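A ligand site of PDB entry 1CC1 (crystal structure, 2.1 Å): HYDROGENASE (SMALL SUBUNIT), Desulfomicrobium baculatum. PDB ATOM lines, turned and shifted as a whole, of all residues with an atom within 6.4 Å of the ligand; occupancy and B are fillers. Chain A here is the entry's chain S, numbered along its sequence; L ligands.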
ATOM      1  N   ILE A 207      22.478  31.771 -29.418  1.00  0.00           N
ATOM      2  CA  ILE A 207      21.407  31.269 -28.551  1.00  0.00           C
ATOM      3  C   ILE A 207      21.889  31.091 -27.115  1.00  0.00           C
ATOM      4  O   ILE A 207      21.291  31.588 -26.156  1.00  0.00           O
ATOM      5  CB  ILE A 207      20.890  29.880 -29.058  1.00  0.00           C
ATOM      6  CG1 ILE A 207      20.389  29.971 -30.512  1.00  0.00           C
ATOM      7  CG2 ILE A 207      19.871  29.295 -28.043  1.00  0.00           C
ATOM      8  CD1 ILE A 207      18.897  30.126 -30.703  1.00  0.00           C
ATOM      9  N   HIS A 208      22.969  30.332 -26.986  1.00  0.00           N
ATOM     10  CA  HIS A 208      23.548  30.008 -25.683  1.00  0.00           C
ATOM     11  C   HIS A 208      23.883  31.251 -24.849  1.00  0.00           C
ATOM     12  O   HIS A 208      23.502  31.334 -23.683  1.00  0.00           O
ATOM     13  CB  HIS A 208      24.777  29.107 -25.889  1.00  0.00           C
ATOM     14  CG  HIS A 208      25.452  28.690 -24.625  1.00  0.00           C
ATOM     15  ND1 HIS A 208      24.914  27.747 -23.784  1.00  0.00           N
ATOM     16  CD2 HIS A 208      26.647  29.112 -24.106  1.00  0.00           C
ATOM     17  CE1 HIS A 208      25.773  27.605 -22.792  1.00  0.00           C
ATOM     18  NE2 HIS A 208      26.837  28.410 -22.949  1.00  0.00           N
ATOM     19  N   GLU A 209      24.515  32.254 -25.449  1.00  0.00           N
ATOM     20  CA  GLU A 209      24.892  33.489 -24.744  1.00  0.00           C
ATOM     21  C   GLU A 209      23.664  34.260 -24.220  1.00  0.00           C
ATOM     22  O   GLU A 209      23.701  34.863 -23.143  1.00  0.00           O
ATOM     23  CB  GLU A 209      25.756  34.370 -25.665  1.00  0.00           C
ATOM     24  CG  GLU A 209      27.208  33.876 -25.740  1.00  0.00           C
ATOM     25  CD  GLU A 209      28.055  34.486 -26.853  1.00  0.00           C
ATOM     26  OE1 GLU A 209      27.710  35.575 -27.371  1.00  0.00           O
ATOM     27  OE2 GLU A 209      29.088  33.868 -27.221  1.00  0.00           O
ATOM     28  N   CYS A 211      20.734  32.664 -23.645  1.00  0.00           N
ATOM     29  CA  CYS A 211      19.828  31.703 -23.074  1.00  0.00           C
ATOM     30  C   CYS A 211      19.515  31.909 -21.596  1.00  0.00           C
ATOM     31  O   CYS A 211      20.398  32.237 -20.804  1.00  0.00           O
ATOM     32  CB  CYS A 211      20.331  30.294 -23.313  1.00  0.00           C
ATOM     33  SG  CYS A 211      19.147  29.032 -22.757  1.00  0.00           S
ATOM     34  N   PRO A 212      18.237  31.734 -21.209  1.00  0.00           N
ATOM     35  CA  PRO A 212      17.829  31.901 -19.805  1.00  0.00           C
ATOM     36  C   PRO A 212      18.381  30.809 -18.864  1.00  0.00           C
ATOM     37  O   PRO A 212      18.378  30.981 -17.648  1.00  0.00           O
ATOM     38  CB  PRO A 212      16.296  31.950 -19.881  1.00  0.00           C
ATOM     39  CG  PRO A 212      15.974  31.155 -21.109  1.00  0.00           C
ATOM     40  CD  PRO A 212      17.053  31.576 -22.084  1.00  0.00           C
ATOM     41  N   TYR A 213      18.859  29.712 -19.446  1.00  0.00           N
ATOM     42  CA  TYR A 213      19.425  28.601 -18.676  1.00  0.00           C
ATOM     43  C   TYR A 213      20.942  28.752 -18.509  1.00  0.00           C
ATOM     44  O   TYR A 213      21.580  27.889 -17.901  1.00  0.00           O
ATOM     45  CB  TYR A 213      19.169  27.269 -19.386  1.00  0.00           C
ATOM     46  CG  TYR A 213      17.731  26.810 -19.413  1.00  0.00           C
ATOM     47  CD1 TYR A 213      17.239  25.975 -18.425  1.00  0.00           C
ATOM     48  CD2 TYR A 213      16.893  27.164 -20.465  1.00  0.00           C
ATOM     49  CE1 TYR A 213      15.931  25.497 -18.478  1.00  0.00           C
ATOM     50  CE2 TYR A 213      15.599  26.694 -20.535  1.00  0.00           C
ATOM     51  CZ  TYR A 213      15.118  25.854 -19.541  1.00  0.00           C
ATOM     52  OH  TYR A 213      13.835  25.377 -19.606  1.00  0.00           O
ATOM     53  N   LEU A 214      21.519  29.815 -19.066  1.00  0.00           N
ATOM     54  CA  LEU A 214      22.957  30.042 -18.989  1.00  0.00           C
ATOM     55  C   LEU A 214      23.572  29.973 -17.590  1.00  0.00           C
ATOM     56  O   LEU A 214      24.680  29.445 -17.436  1.00  0.00           O
ATOM     57  CB  LEU A 214      23.328  31.361 -19.669  1.00  0.00           C
ATOM     58  CG  LEU A 214      24.832  31.567 -19.920  1.00  0.00           C
ATOM     59  CD1 LEU A 214      25.364  30.523 -20.896  1.00  0.00           C
ATOM     60  CD2 LEU A 214      25.052  32.970 -20.458  1.00  0.00           C
ATOM     61  N   ASP A 215      22.885  30.508 -16.581  1.00  0.00           N
ATOM     62  CA  ASP A 215      23.403  30.472 -15.216  1.00  0.00           C
ATOM     63  C   ASP A 215      23.443  29.054 -14.676  1.00  0.00           C
ATOM     64  O   ASP A 215      24.342  28.694 -13.928  1.00  0.00           O
ATOM     65  CB  ASP A 215      22.581  31.383 -14.294  1.00  0.00           C
ATOM     66  CG  ASP A 215      21.087  31.021 -14.258  1.00  0.00           C
ATOM     67  OD1 ASP A 215      20.565  30.418 -15.219  1.00  0.00           O
ATOM     68  OD2 ASP A 215      20.428  31.374 -13.248  1.00  0.00           O
ATOM     69  N   LYS A 216      22.475  28.236 -15.082  1.00  0.00           N
ATOM     70  CA  LYS A 216      22.449  26.852 -14.646  1.00  0.00           C
ATOM     71  C   LYS A 216      23.624  26.142 -15.305  1.00  0.00           C
ATOM     72  O   LYS A 216      24.352  25.388 -14.659  1.00  0.00           O
ATOM     73  CB  LYS A 216      21.113  26.189 -15.014  1.00  0.00           C
ATOM     74  CG  LYS A 216      19.896  26.824 -14.352  1.00  0.00           C
ATOM     75  CD  LYS A 216      20.087  26.867 -12.841  1.00  0.00           C
ATOM     76  CE  LYS A 216      19.279  27.990 -12.174  1.00  0.00           C
ATOM     77  NZ  LYS A 216      19.861  28.384 -10.849  1.00  0.00           N
ATOM     78  N   TYR A 217      23.862  26.478 -16.569  1.00  0.00           N
ATOM     79  CA  TYR A 217      24.964  25.921 -17.349  1.00  0.00           C
ATOM     80  C   TYR A 217      26.294  26.225 -16.675  1.00  0.00           C
ATOM     81  O   TYR A 217      27.094  25.335 -16.394  1.00  0.00           O
ATOM     82  CB  TYR A 217      24.957  26.529 -18.762  1.00  0.00           C
ATOM     83  CG  TYR A 217      26.142  26.140 -19.626  1.00  0.00           C
ATOM     84  CD1 TYR A 217      26.097  25.006 -20.427  1.00  0.00           C
ATOM     85  CD2 TYR A 217      27.310  26.896 -19.618  1.00  0.00           C
ATOM     86  CE1 TYR A 217      27.191  24.634 -21.196  1.00  0.00           C
ATOM     87  CE2 TYR A 217      28.402  26.531 -20.375  1.00  0.00           C
ATOM     88  CZ  TYR A 217      28.331  25.396 -21.164  1.00  0.00           C
ATOM     89  OH  TYR A 217      29.425  25.017 -21.920  1.00  0.00           O
ATOM     90  N   PHE A 222      22.748  20.361 -14.964  1.00  0.00           N
ATOM     91  CA  PHE A 222      22.180  19.837 -16.197  1.00  0.00           C
ATOM     92  C   PHE A 222      20.985  18.896 -15.969  1.00  0.00           C
ATOM     93  O   PHE A 222      21.045  18.038 -15.093  1.00  0.00           O
ATOM     94  CB  PHE A 222      23.276  19.103 -16.961  1.00  0.00           C
ATOM     95  CG  PHE A 222      24.467  19.962 -17.292  1.00  0.00           C
ATOM     96  CD1 PHE A 222      24.361  20.933 -18.266  1.00  0.00           C
ATOM     97  CD2 PHE A 222      25.685  19.802 -16.619  1.00  0.00           C
ATOM     98  CE1 PHE A 222      25.431  21.753 -18.592  1.00  0.00           C
ATOM     99  CE2 PHE A 222      26.775  20.625 -16.934  1.00  0.00           C
ATOM    100  CZ  PHE A 222      26.642  21.600 -17.917  1.00  0.00           C
ATOM    101  N   GLY A 230      17.178  22.169 -15.029  1.00  0.00           N
ATOM    102  CA  GLY A 230      18.533  22.427 -15.457  1.00  0.00           C
ATOM    103  C   GLY A 230      18.707  22.721 -16.931  1.00  0.00           C
ATOM    104  O   GLY A 230      17.771  22.615 -17.737  1.00  0.00           O
ATOM    105  N   CYS A 231      19.928  23.120 -17.274  1.00  0.00           N
ATOM    106  CA  CYS A 231      20.313  23.414 -18.647  1.00  0.00           C
ATOM    107  C   CYS A 231      20.151  22.121 -19.469  1.00  0.00           C
ATOM    108  O   CYS A 231      20.270  21.014 -18.934  1.00  0.00           O
ATOM    109  CB  CYS A 231      21.754  23.923 -18.625  1.00  0.00           C
ATOM    110  SG  CYS A 231      22.721  23.691 -20.130  1.00  0.00           S
ATOM    111  N   LYS A 232      19.830  22.282 -20.747  1.00  0.00           N
ATOM    112  CA  LYS A 232      19.593  21.164 -21.670  1.00  0.00           C
ATOM    113  C   LYS A 232      20.805  20.639 -22.427  1.00  0.00           C
ATOM    114  O   LYS A 232      20.670  19.779 -23.316  1.00  0.00           O
ATOM    115  CB  LYS A 232      18.525  21.557 -22.706  1.00  0.00           C
ATOM    116  CG  LYS A 232      17.329  22.318 -22.151  1.00  0.00           C
ATOM    117  CD  LYS A 232      16.593  21.479 -21.116  1.00  0.00           C
ATOM    118  CE  LYS A 232      15.306  22.143 -20.667  1.00  0.00           C
ATOM    119  NZ  LYS A 232      14.303  22.191 -21.763  1.00  0.00           N
ATOM    120  N   ALA A 233      21.988  21.153 -22.087  1.00  0.00           N
ATOM    121  CA  ALA A 233      23.253  20.764 -22.712  1.00  0.00           C
ATOM    122  C   ALA A 233      23.416  19.252 -22.874  1.00  0.00           C
ATOM    123  O   ALA A 233      23.643  18.769 -23.972  1.00  0.00           O
ATOM    124  CB  ALA A 233      24.418  21.335 -21.937  1.00  0.00           C
ATOM    125  N   GLU A 234      23.232  18.518 -21.783  1.00  0.00           N
ATOM    126  CA  GLU A 234      23.354  17.057 -21.808  1.00  0.00           C
ATOM    127  C   GLU A 234      22.312  16.338 -22.641  1.00  0.00           C
ATOM    128  O   GLU A 234      22.512  15.183 -23.023  1.00  0.00           O
ATOM    129  CB  GLU A 234      23.289  16.508 -20.388  1.00  0.00           C
ATOM    130  CG  GLU A 234      24.595  16.449 -19.665  1.00  0.00           C
ATOM    131  CD  GLU A 234      24.389  15.980 -18.252  1.00  0.00           C
ATOM    132  OE1 GLU A 234      25.055  16.529 -17.342  1.00  0.00           O
ATOM    133  OE2 GLU A 234      23.547  15.082 -18.036  1.00  0.00           O
ATOM    134  N   CYS A 237      21.355  19.785 -26.620  1.00  0.00           N
ATOM    135  CA  CYS A 237      21.208  21.177 -27.042  1.00  0.00           C
ATOM    136  C   CYS A 237      22.375  21.760 -27.861  1.00  0.00           C
ATOM    137  O   CYS A 237      23.543  21.723 -27.428  1.00  0.00           O
ATOM    138  CB  CYS A 237      20.928  22.065 -25.818  1.00  0.00           C
ATOM    139  SG  CYS A 237      20.515  23.752 -26.315  1.00  0.00           S
ATOM    140  N   LYS A 238      22.052  22.287 -29.043  1.00  0.00           N
ATOM    141  CA  LYS A 238      23.080  22.865 -29.907  1.00  0.00           C
ATOM    142  C   LYS A 238      23.071  24.384 -29.883  1.00  0.00           C
ATOM    143  O   LYS A 238      23.595  25.004 -30.781  1.00  0.00           O
ATOM    144  CB  LYS A 238      22.929  22.387 -31.359  1.00  0.00           C
ATOM    145  CG  LYS A 238      22.823  20.888 -31.541  1.00  0.00           C
ATOM    146  CD  LYS A 238      23.962  20.126 -30.853  1.00  0.00           C
ATOM    147  CE  LYS A 238      23.965  18.635 -31.251  1.00  0.00           C
ATOM    148  NZ  LYS A 238      22.778  17.859 -30.785  1.00  0.00           N
ATOM    149  N   GLY A 239      22.474  24.970 -28.842  1.00  0.00           N
ATOM    150  CA  GLY A 239      22.448  26.413 -28.717  1.00  0.00           C
ATOM    151  C   GLY A 239      23.832  27.044 -28.733  1.00  0.00           C
ATOM    152  O   GLY A 239      24.016  28.124 -29.309  1.00  0.00           O
ATOM    153  N   PRO A 240      24.845  26.434 -28.076  1.00  0.00           N
ATOM    154  CA  PRO A 240      26.197  27.012 -28.084  1.00  0.00           C
ATOM    155  C   PRO A 240      26.762  27.326 -29.487  1.00  0.00           C
ATOM    156  O   PRO A 240      27.476  28.330 -29.662  1.00  0.00           O
ATOM    157  CB  PRO A 240      27.020  25.927 -27.380  1.00  0.00           C
ATOM    158  CG  PRO A 240      26.055  25.359 -26.381  1.00  0.00           C
ATOM    159  CD  PRO A 240      24.783  25.240 -27.206  1.00  0.00           C
ATOM    160  N   TRP A 257       9.381  27.980 -26.815  1.00  0.00           N
ATOM    161  CA  TRP A 257      10.511  27.860 -27.740  1.00  0.00           C
ATOM    162  C   TRP A 257      11.191  26.504 -27.513  1.00  0.00           C
ATOM    163  O   TRP A 257      10.929  25.831 -26.512  1.00  0.00           O
ATOM    164  CB  TRP A 257      11.467  29.068 -27.722  1.00  0.00           C
ATOM    165  CG  TRP A 257      12.304  29.245 -26.500  1.00  0.00           C
ATOM    166  CD1 TRP A 257      11.871  29.363 -25.224  1.00  0.00           C
ATOM    167  CD2 TRP A 257      13.748  29.400 -26.453  1.00  0.00           C
ATOM    168  NE1 TRP A 257      12.935  29.587 -24.376  1.00  0.00           N
ATOM    169  CE2 TRP A 257      14.094  29.613 -25.104  1.00  0.00           C
ATOM    170  CE3 TRP A 257      14.759  29.383 -27.419  1.00  0.00           C
ATOM    171  CZ2 TRP A 257      15.411  29.799 -24.692  1.00  0.00           C
ATOM    172  CZ3 TRP A 257      16.085  29.578 -27.001  1.00  0.00           C
ATOM    173  CH2 TRP A 257      16.392  29.780 -25.655  1.00  0.00           C
ATOM    174  N   VAL A 259      14.261  25.426 -26.771  1.00  0.00           N
ATOM    175  CA  VAL A 259      15.084  25.182 -25.588  1.00  0.00           C
ATOM    176  C   VAL A 259      14.286  24.987 -24.296  1.00  0.00           C
ATOM    177  O   VAL A 259      14.589  24.067 -23.528  1.00  0.00           O
ATOM    178  CB  VAL A 259      16.216  26.245 -25.431  1.00  0.00           C
ATOM    179  CG1 VAL A 259      17.035  25.976 -24.156  1.00  0.00           C
ATOM    180  CG2 VAL A 259      17.131  26.198 -26.638  1.00  0.00           C
ATOM    181  N   ALA A 262      12.424  21.557 -24.998  1.00  0.00           N
ATOM    182  CA  ALA A 262      13.333  20.411 -25.169  1.00  0.00           C
ATOM    183  C   ALA A 262      14.799  20.851 -25.353  1.00  0.00           C
ATOM    184  O   ALA A 262      15.497  21.164 -24.375  1.00  0.00           O
ATOM    185  CB  ALA A 262      12.868  19.556 -26.359  1.00  0.00           C
ATOM    186  N   CYS A 264      17.601  22.867 -28.476  1.00  0.00           N
ATOM    187  CA  CYS A 264      17.746  23.586 -29.735  1.00  0.00           C
ATOM    188  C   CYS A 264      18.420  22.549 -30.657  1.00  0.00           C
ATOM    189  O   CYS A 264      19.275  21.791 -30.191  1.00  0.00           O
ATOM    190  CB  CYS A 264      18.654  24.794 -29.584  1.00  0.00           C
ATOM    191  SG  CYS A 264      19.220  25.492 -31.182  1.00  0.00           S
HETATM  192 FE1  LIG L   1      21.211  25.038 -24.558  1.00  0.00          FE
HETATM  193 FE2  LIG L   1      23.241  26.752 -23.584  1.00  0.00          FE
HETATM  194 FE3  LIG L   1      22.047  25.166 -21.761  1.00  0.00          FE
HETATM  195 FE4  LIG L   1      20.621  27.251 -22.912  1.00  0.00          FE
HETATM  196  S1  LIG L   1      22.460  27.384 -21.445  1.00  0.00           S
HETATM  197  S2  LIG L   1      19.817  25.153 -22.580  1.00  0.00           S
HETATM  198  S3  LIG L   1      21.537  27.268 -25.074  1.00  0.00           S
HETATM  199  S4  LIG L   1      23.266  24.408 -23.653  1.00  0.00           S
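An iron atom (FE2) of the ligand is bound by a ring nitrogen (ND1) of His 208 (2.0 Å). An iron atom (FE1) of the ligand is bound by the side-chain sulfur (SG) of Cys 237. FE3 of the ligand is bound by SG of Cys 231 (2.3 Å). SG of Cys 211 is bound to FE4 of the ligand (2.3 Å). N of Lys 232 sits close to S2 of the ligand, 3.4 Å away. The backbone NH (N) of Leu 214 sits close to a sulfur (S1) of the ligand, 3.5 Å away.
The backbone carbonyl oxygen of Tyr 213 lies close to a sulfur (S1) of the ligand (3.7 Å). Residues that only touch the ligand: Ile 207 (3.96 Å), Tyr 217 (3.8 Å), Ala 233 (3.7 Å), Gly 239 (3.9 Å), Pro 240 (3.95 Å) and Val 259 (3.3 Å).
The backbone NH (N) of His 208 lies within hydrogen-bond range of the backbone carbonyl oxygen (O) of Gly 239 (3.4 Å). The backbone NH (N) of Cys 237 sits at hydrogen-bond distance from the backbone carbonyl oxygen (O) of Lys 232. The side-chain sulfur (SG) of Cys 237 lies close to the backbone NH (N) of Gly 239, at 3.4 Å. SG of Cys 237 lies close to N of Cys 264 (3.7 Å). The backbone NH (N) of Ala 233 sits close to the side-chain sulfur (SG) of Cys 231 (3.3 Å). The side-chain sulfur (SG) of Cys 211 lies close to the backbone NH (N) of Tyr 213. The backbone carbonyl oxygen of Val 259 sits at hydrogen-bond distance from the side-chain amino group of Lys 232 (2.6 Å). NZ of Lys 232 is in hydrogen-bond range of O of Ala 262, 3.1 Å away.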
